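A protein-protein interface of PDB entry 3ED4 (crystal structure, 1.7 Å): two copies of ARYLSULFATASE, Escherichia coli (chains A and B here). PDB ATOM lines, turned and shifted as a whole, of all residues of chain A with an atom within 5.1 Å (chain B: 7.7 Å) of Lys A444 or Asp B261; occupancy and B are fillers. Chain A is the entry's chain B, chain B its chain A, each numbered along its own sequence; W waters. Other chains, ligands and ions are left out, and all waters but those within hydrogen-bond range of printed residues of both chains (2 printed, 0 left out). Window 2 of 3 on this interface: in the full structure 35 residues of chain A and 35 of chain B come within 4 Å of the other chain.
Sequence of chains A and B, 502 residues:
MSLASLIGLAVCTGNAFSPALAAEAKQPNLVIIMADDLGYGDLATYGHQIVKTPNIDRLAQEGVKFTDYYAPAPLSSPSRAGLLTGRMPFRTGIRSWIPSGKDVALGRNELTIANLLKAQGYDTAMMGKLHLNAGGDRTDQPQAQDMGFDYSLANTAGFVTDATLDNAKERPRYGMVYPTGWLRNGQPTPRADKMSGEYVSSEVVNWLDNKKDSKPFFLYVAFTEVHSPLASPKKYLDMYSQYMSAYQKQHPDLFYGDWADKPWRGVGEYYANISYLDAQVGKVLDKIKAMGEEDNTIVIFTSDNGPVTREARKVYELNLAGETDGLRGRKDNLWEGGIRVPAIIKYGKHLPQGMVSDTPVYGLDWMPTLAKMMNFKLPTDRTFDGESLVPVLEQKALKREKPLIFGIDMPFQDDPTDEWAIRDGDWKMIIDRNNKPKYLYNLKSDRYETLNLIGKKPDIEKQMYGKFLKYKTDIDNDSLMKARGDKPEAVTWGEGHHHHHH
Water W2 lies within hydrogen-bond range of the side-chain carboxylate (OD1) of Asp A446 and the backbone carbonyl oxygen (O) of Ala B260. Water W1 bridges N of Trp B264 (2.9 Å) and NH2 of Arg A447 (3.4 Å).
O of Lys A444 touches CB of Asp B261, 3.4 Å away. Ala B260 touches Ser A445. CB of Asp B261 touches O of Ser A445 (3.6 Å). Ala B260 touches Asp A446. CD of Arg A447 touches O of Lys B262, 3.7 Å away. Trp B264 touches Arg A447 (N to NH1, 3.8 Å).
Asn A442 touches none of the printed residues of chain B. Of the printed residues of chain B, Asp A446 touches Ala B260 (3.6 Å). Tyr B247 touches none of the printed residues of chain A. Of the printed residues of chain A, Lys B262 touches Arg A447 (3.7 Å). Printed residues of chain A within 4 Å of Trp B264: Arg A447 (3.8 Å). The nearest residue of chain B that does not touch Lys A444 is Ala B260 (5.7 Å). The nearest residue of chain A that does not touch Asp B261 is Arg A447 (4.5 Å).
No position is printed for both chains.
N of Arg A447 lies within hydrogen-bond range of O of Ala B260, 2.9 Å away.
Printed residues of chain A that touch a printed residue of chain B: Lys A444, Ser A445, Asp A446 and Arg A447. Of the 13 printed residues of chain B, 4 touch a printed residue of chain A. Along chain B the printed residues that touch a printed residue of chain A span positions 260 to 264. Among the printed residues, 7 pairs touch across the chains.
The backbone carbonyl oxygen of Asp B258 sits at hydrogen-bond distance from the side-chain amino group of Lys B262. The side-chain amino group (NZ) of Lys B262 is in salt-bridge range of the side-chain carboxylate (OD1) of Asp B261. The backbone NH (N) of Lys A444 lies within hydrogen-bond range of the side-chain amide oxygen (OD1) of Asn A442 (3.0 Å). The side-chain amide oxygen (OD1) of Asn A442 is in hydrogen-bond range of the backbone NH (N) of Ser A445 (3.3 Å).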
ATOM      1  N   ASP A 426     -10.388   9.923  20.342  1.00  0.00           N
ATOM      2  CA  ASP A 426     -10.312   8.927  21.405  1.00  0.00           C
ATOM      3  C   ASP A 426     -11.267   9.246  22.578  1.00  0.00           C
ATOM      4  O   ASP A 426     -11.398   8.445  23.502  1.00  0.00           O
ATOM      5  CB  ASP A 426      -8.877   8.814  21.941  1.00  0.00           C
ATOM      6  CG  ASP A 426      -7.840   8.560  20.850  1.00  0.00           C
ATOM      7  OD1 ASP A 426      -8.151   7.914  19.828  1.00  0.00           O
ATOM      8  OD2 ASP A 426      -6.685   8.991  21.040  1.00  0.00           O
ATOM      9  N   ASN A 442     -11.089   8.486  27.899  1.00  0.00           N
ATOM     10  CA  ASN A 442     -10.198   8.384  26.753  1.00  0.00           C
ATOM     11  C   ASN A 442     -10.090   6.910  26.417  1.00  0.00           C
ATOM     12  O   ASN A 442      -9.391   6.160  27.108  1.00  0.00           O
ATOM     13  CB  ASN A 442      -8.817   8.963  27.069  1.00  0.00           C
ATOM     14  CG  ASN A 442      -7.910   9.026  25.849  1.00  0.00           C
ATOM     15  OD1 ASN A 442      -7.664   8.022  25.182  1.00  0.00           O
ATOM     16  ND2 ASN A 442      -7.388  10.212  25.571  1.00  0.00           N
ATOM     17  N   LEU A 443     -10.757   6.489  25.348  1.00  0.00           N
ATOM     18  CA  LEU A 443     -10.761   5.065  24.986  1.00  0.00           C
ATOM     19  C   LEU A 443      -9.412   4.461  24.591  1.00  0.00           C
ATOM     20  O   LEU A 443      -9.239   3.242  24.673  1.00  0.00           O
ATOM     21  CB  LEU A 443     -11.809   4.771  23.912  1.00  0.00           C
ATOM     22  CG  LEU A 443     -13.240   5.015  24.382  1.00  0.00           C
ATOM     23  CD1 LEU A 443     -14.241   4.880  23.217  1.00  0.00           C
ATOM     24  CD2 LEU A 443     -13.600   4.088  25.555  1.00  0.00           C
ATOM     25  N   LYS A 444      -8.470   5.310  24.173  1.00  0.00           N
ATOM     26  CA  LYS A 444      -7.113   4.873  23.825  1.00  0.00           C
ATOM     27  C   LYS A 444      -6.323   4.407  25.061  1.00  0.00           C
ATOM     28  O   LYS A 444      -5.576   3.436  24.984  1.00  0.00           O
ATOM     29  CB  LYS A 444      -6.357   5.992  23.083  1.00  0.00           C
ATOM     30  CG  LYS A 444      -5.010   5.580  22.483  1.00  0.00           C
ATOM     31  CD  LYS A 444      -4.245   6.807  21.991  1.00  0.00           C
ATOM     32  CE  LYS A 444      -3.158   6.429  20.999  1.00  0.00           C
ATOM     33  NZ  LYS A 444      -3.735   6.111  19.659  1.00  0.00           N
ATOM     34  N   SER A 445      -6.490   5.105  26.184  1.00  0.00           N
ATOM     35  CA  SER A 445      -5.801   4.743  27.431  1.00  0.00           C
ATOM     36  C   SER A 445      -6.673   3.943  28.408  1.00  0.00           C
ATOM     37  O   SER A 445      -6.184   3.457  29.432  1.00  0.00           O
ATOM     38  CB  SER A 445      -5.248   5.999  28.125  1.00  0.00           C
ATOM     39  OG  SER A 445      -6.253   6.972  28.309  1.00  0.00           O
ATOM     40  N   ASP A 446      -7.956   3.802  28.080  1.00  0.00           N
ATOM     41  CA  ASP A 446      -8.937   3.176  28.966  1.00  0.00           C
ATOM     42  C   ASP A 446      -9.957   2.431  28.095  1.00  0.00           C
ATOM     43  O   ASP A 446     -11.090   2.877  27.936  1.00  0.00           O
ATOM     44  CB  ASP A 446      -9.614   4.270  29.823  1.00  0.00           C
ATOM     45  CG  ASP A 446     -10.674   3.739  30.814  1.00  0.00           C
ATOM     46  OD1 ASP A 446     -10.650   2.561  31.218  1.00  0.00           O
ATOM     47  OD2 ASP A 446     -11.521   4.560  31.218  1.00  0.00           O
ATOM     48  N   ARG A 447      -9.530   1.312  27.522  1.00  0.00           N
ATOM     49  CA  ARG A 447     -10.394   0.471  26.675  1.00  0.00           C
ATOM     50  C   ARG A 447     -11.689   0.019  27.396  1.00  0.00           C
ATOM     51  O   ARG A 447     -12.741  -0.121  26.780  1.00  0.00           O
ATOM     52  CB  ARG A 447      -9.616  -0.754  26.167  1.00  0.00           C
ATOM     53  CG  ARG A 447     -10.316  -1.519  25.040  1.00  0.00           C
ATOM     54  CD  ARG A 447      -9.551  -2.751  24.563  1.00  0.00           C
ATOM     55  NE  ARG A 447     -10.302  -3.388  23.477  1.00  0.00           N
ATOM     56  CZ  ARG A 447     -11.002  -4.516  23.585  1.00  0.00           C
ATOM     57  NH1 ARG A 447     -11.018  -5.196  24.727  1.00  0.00           N
ATOM     58  NH2 ARG A 447     -11.667  -4.976  22.534  1.00  0.00           N
ATOM     59  N   PRO B 172       5.653  -1.302  29.135  1.00  0.00           N
ATOM     60  CA  PRO B 172       4.912  -2.087  30.129  1.00  0.00           C
ATOM     61  C   PRO B 172       5.815  -2.923  31.053  1.00  0.00           C
ATOM     62  O   PRO B 172       7.012  -3.079  30.780  1.00  0.00           O
ATOM     63  CB  PRO B 172       4.047  -3.020  29.267  1.00  0.00           C
ATOM     64  CG  PRO B 172       4.411  -2.754  27.828  1.00  0.00           C
ATOM     65  CD  PRO B 172       5.680  -1.982  27.828  1.00  0.00           C
ATOM     66  N   TYR B 247      -3.394 -12.102  22.316  1.00  0.00           N
ATOM     67  CA  TYR B 247      -2.614 -11.092  23.029  1.00  0.00           C
ATOM     68  C   TYR B 247      -2.025 -11.630  24.340  1.00  0.00           C
ATOM     69  O   TYR B 247      -0.865 -11.341  24.673  1.00  0.00           O
ATOM     70  CB  TYR B 247      -3.422  -9.827  23.301  1.00  0.00           C
ATOM     71  CG  TYR B 247      -2.571  -8.729  23.889  1.00  0.00           C
ATOM     72  CD1 TYR B 247      -1.808  -7.896  23.065  1.00  0.00           C
ATOM     73  CD2 TYR B 247      -2.498  -8.539  25.274  1.00  0.00           C
ATOM     74  CE1 TYR B 247      -1.016  -6.889  23.603  1.00  0.00           C
ATOM     75  CE2 TYR B 247      -1.705  -7.551  25.814  1.00  0.00           C
ATOM     76  CZ  TYR B 247      -0.969  -6.728  24.979  1.00  0.00           C
ATOM     77  OH  TYR B 247      -0.186  -5.743  25.537  1.00  0.00           O
ATOM     78  N   LEU B 254       2.395 -10.024  31.476  1.00  0.00           N
ATOM     79  CA  LEU B 254       2.072  -8.595  31.554  1.00  0.00           C
ATOM     80  C   LEU B 254       1.413  -8.239  32.888  1.00  0.00           C
ATOM     81  O   LEU B 254       0.395  -8.827  33.264  1.00  0.00           O
ATOM     82  CB  LEU B 254       1.194  -8.152  30.372  1.00  0.00           C
ATOM     83  CG  LEU B 254       0.783  -6.677  30.311  1.00  0.00           C
ATOM     84  CD1 LEU B 254       2.002  -5.783  30.175  1.00  0.00           C
ATOM     85  CD2 LEU B 254      -0.198  -6.427  29.168  1.00  0.00           C
ATOM     86  N   GLY B 257      -1.176  -3.882  36.350  1.00  0.00           N
ATOM     87  CA  GLY B 257      -1.121  -2.427  36.465  1.00  0.00           C
ATOM     88  C   GLY B 257      -1.081  -1.738  35.109  1.00  0.00           C
ATOM     89  O   GLY B 257      -1.363  -0.531  34.990  1.00  0.00           O
ATOM     90  N   ASP B 258      -0.755  -2.530  34.089  1.00  0.00           N
ATOM     91  CA  ASP B 258      -0.624  -2.064  32.722  1.00  0.00           C
ATOM     92  C   ASP B 258      -1.688  -2.634  31.753  1.00  0.00           C
ATOM     93  O   ASP B 258      -1.479  -2.643  30.546  1.00  0.00           O
ATOM     94  CB  ASP B 258       0.798  -2.365  32.223  1.00  0.00           C
ATOM     95  CG  ASP B 258       1.874  -1.708  33.085  1.00  0.00           C
ATOM     96  OD1 ASP B 258       1.679  -0.558  33.530  1.00  0.00           O
ATOM     97  OD2 ASP B 258       2.912  -2.352  33.320  1.00  0.00           O
ATOM     98  N   TRP B 259      -2.832  -3.071  32.286  1.00  0.00           N
ATOM     99  CA  TRP B 259      -3.877  -3.721  31.477  1.00  0.00           C
ATOM    100  C   TRP B 259      -4.940  -2.789  30.873  1.00  0.00           C
ATOM    101  O   TRP B 259      -5.641  -3.200  29.947  1.00  0.00           O
ATOM    102  CB  TRP B 259      -4.583  -4.795  32.305  1.00  0.00           C
ATOM    103  CG  TRP B 259      -3.817  -6.076  32.504  1.00  0.00           C
ATOM    104  CD1 TRP B 259      -2.532  -6.364  32.083  1.00  0.00           C
ATOM    105  CD2 TRP B 259      -4.279  -7.242  33.206  1.00  0.00           C
ATOM    106  NE1 TRP B 259      -2.185  -7.638  32.471  1.00  0.00           N
ATOM    107  CE2 TRP B 259      -3.235  -8.199  33.159  1.00  0.00           C
ATOM    108  CE3 TRP B 259      -5.474  -7.570  33.869  1.00  0.00           C
ATOM    109  CZ2 TRP B 259      -3.346  -9.451  33.759  1.00  0.00           C
ATOM    110  CZ3 TRP B 259      -5.585  -8.822  34.456  1.00  0.00           C
ATOM    111  CH2 TRP B 259      -4.527  -9.753  34.388  1.00  0.00           C
ATOM    112  N   ALA B 260      -5.051  -1.550  31.375  1.00  0.00           N
ATOM    113  CA  ALA B 260      -6.168  -0.641  31.002  1.00  0.00           C
ATOM    114  C   ALA B 260      -6.323  -0.328  29.509  1.00  0.00           C
ATOM    115  O   ALA B 260      -7.449  -0.096  29.025  1.00  0.00           O
ATOM    116  CB  ALA B 260      -6.099   0.646  31.783  1.00  0.00           C
ATOM    117  N   ASP B 261      -5.199  -0.314  28.793  1.00  0.00           N
ATOM    118  CA  ASP B 261      -5.185   0.098  27.394  1.00  0.00           C
ATOM    119  C   ASP B 261      -4.802  -1.051  26.467  1.00  0.00           C
ATOM    120  O   ASP B 261      -4.450  -0.846  25.303  1.00  0.00           O
ATOM    121  CB  ASP B 261      -4.247   1.304  27.216  1.00  0.00           C
ATOM    122  CG  ASP B 261      -2.775   0.960  27.440  1.00  0.00           C
ATOM    123  OD1 ASP B 261      -2.457   0.093  28.290  1.00  0.00           O
ATOM    124  OD2 ASP B 261      -1.928   1.580  26.758  1.00  0.00           O
ATOM    125  N   LYS B 262      -4.884  -2.265  26.997  1.00  0.00           N
ATOM    126  CA  LYS B 262      -4.447  -3.445  26.274  1.00  0.00           C
ATOM    127  C   LYS B 262      -5.649  -4.285  25.834  1.00  0.00           C
ATOM    128  O   LYS B 262      -6.723  -4.174  26.437  1.00  0.00           O
ATOM    129  CB  LYS B 262      -3.503  -4.279  27.146  1.00  0.00           C
ATOM    130  CG  LYS B 262      -2.214  -3.579  27.569  1.00  0.00           C
ATOM    131  CD  LYS B 262      -1.444  -2.961  26.420  1.00  0.00           C
ATOM    132  CE  LYS B 262      -0.053  -2.522  26.890  1.00  0.00           C
ATOM    133  NZ  LYS B 262      -0.156  -1.571  28.023  1.00  0.00           N
ATOM    134  N   PRO B 263      -5.476  -5.114  24.778  1.00  0.00           N
ATOM    135  CA  PRO B 263      -6.512  -6.070  24.377  1.00  0.00           C
ATOM    136  C   PRO B 263      -6.934  -7.038  25.484  1.00  0.00           C
ATOM    137  O   PRO B 263      -6.223  -7.211  26.487  1.00  0.00           O
ATOM    138  CB  PRO B 263      -5.845  -6.854  23.244  1.00  0.00           C
ATOM    139  CG  PRO B 263      -4.853  -5.937  22.688  1.00  0.00           C
ATOM    140  CD  PRO B 263      -4.324  -5.163  23.853  1.00  0.00           C
ATOM    141  N   TRP B 264      -8.103  -7.645  25.292  1.00  0.00           N
ATOM    142  CA  TRP B 264      -8.658  -8.620  26.220  1.00  0.00           C
ATOM    143  C   TRP B 264      -7.741  -9.838  26.297  1.00  0.00           C
ATOM    144  O   TRP B 264      -7.151 -10.238  25.299  1.00  0.00           O
ATOM    145  CB  TRP B 264     -10.037  -9.051  25.724  1.00  0.00           C
ATOM    146  CG  TRP B 264     -10.845  -9.885  26.674  1.00  0.00           C
ATOM    147  CD1 TRP B 264     -11.166  -9.585  27.967  1.00  0.00           C
ATOM    148  CD2 TRP B 264     -11.497 -11.135  26.378  1.00  0.00           C
ATOM    149  NE1 TRP B 264     -11.941 -10.585  28.507  1.00  0.00           N
ATOM    150  CE2 TRP B 264     -12.153 -11.550  27.558  1.00  0.00           C
ATOM    151  CE3 TRP B 264     -11.561 -11.958  25.244  1.00  0.00           C
ATOM    152  CZ2 TRP B 264     -12.910 -12.728  27.622  1.00  0.00           C
ATOM    153  CZ3 TRP B 264     -12.300 -13.149  25.317  1.00  0.00           C
ATOM    154  CH2 TRP B 264     -12.952 -13.523  26.504  1.00  0.00           C
ATOM    155  N   VAL B 315     -10.495  -0.473  37.382  1.00  0.00           N
ATOM    156  CA  VAL B 315      -9.296  -0.801  36.613  1.00  0.00           C
ATOM    157  C   VAL B 315      -8.529  -2.032  37.155  1.00  0.00           C
ATOM    158  O   VAL B 315      -7.786  -2.696  36.418  1.00  0.00           O
ATOM    159  CB  VAL B 315      -8.367   0.457  36.468  1.00  0.00           C
ATOM    160  CG1 VAL B 315      -7.613   0.752  37.774  1.00  0.00           C
ATOM    161  CG2 VAL B 315      -7.416   0.307  35.291  1.00  0.00           C
ATOM    162  N   LEU B 318     -10.086  -5.916  35.706  1.00  0.00           N
ATOM    163  CA  LEU B 318     -10.004  -6.310  34.298  1.00  0.00           C
ATOM    164  C   LEU B 318      -9.583  -7.758  34.084  1.00  0.00           C
ATOM    165  O   LEU B 318      -8.818  -8.326  34.882  1.00  0.00           O
ATOM    166  CB  LEU B 318      -9.054  -5.386  33.519  1.00  0.00           C
ATOM    167  CG  LEU B 318      -9.244  -3.873  33.657  1.00  0.00           C
ATOM    168  CD1 LEU B 318      -8.219  -3.148  32.812  1.00  0.00           C
ATOM    169  CD2 LEU B 318     -10.679  -3.420  33.319  1.00  0.00           C
HETATM  170  O   HOH W   1      -9.188  -7.255  22.600  1.00  0.00           O
HETATM  171  O   HOH W   2      -9.592   0.286  30.969  1.00  0.00           O
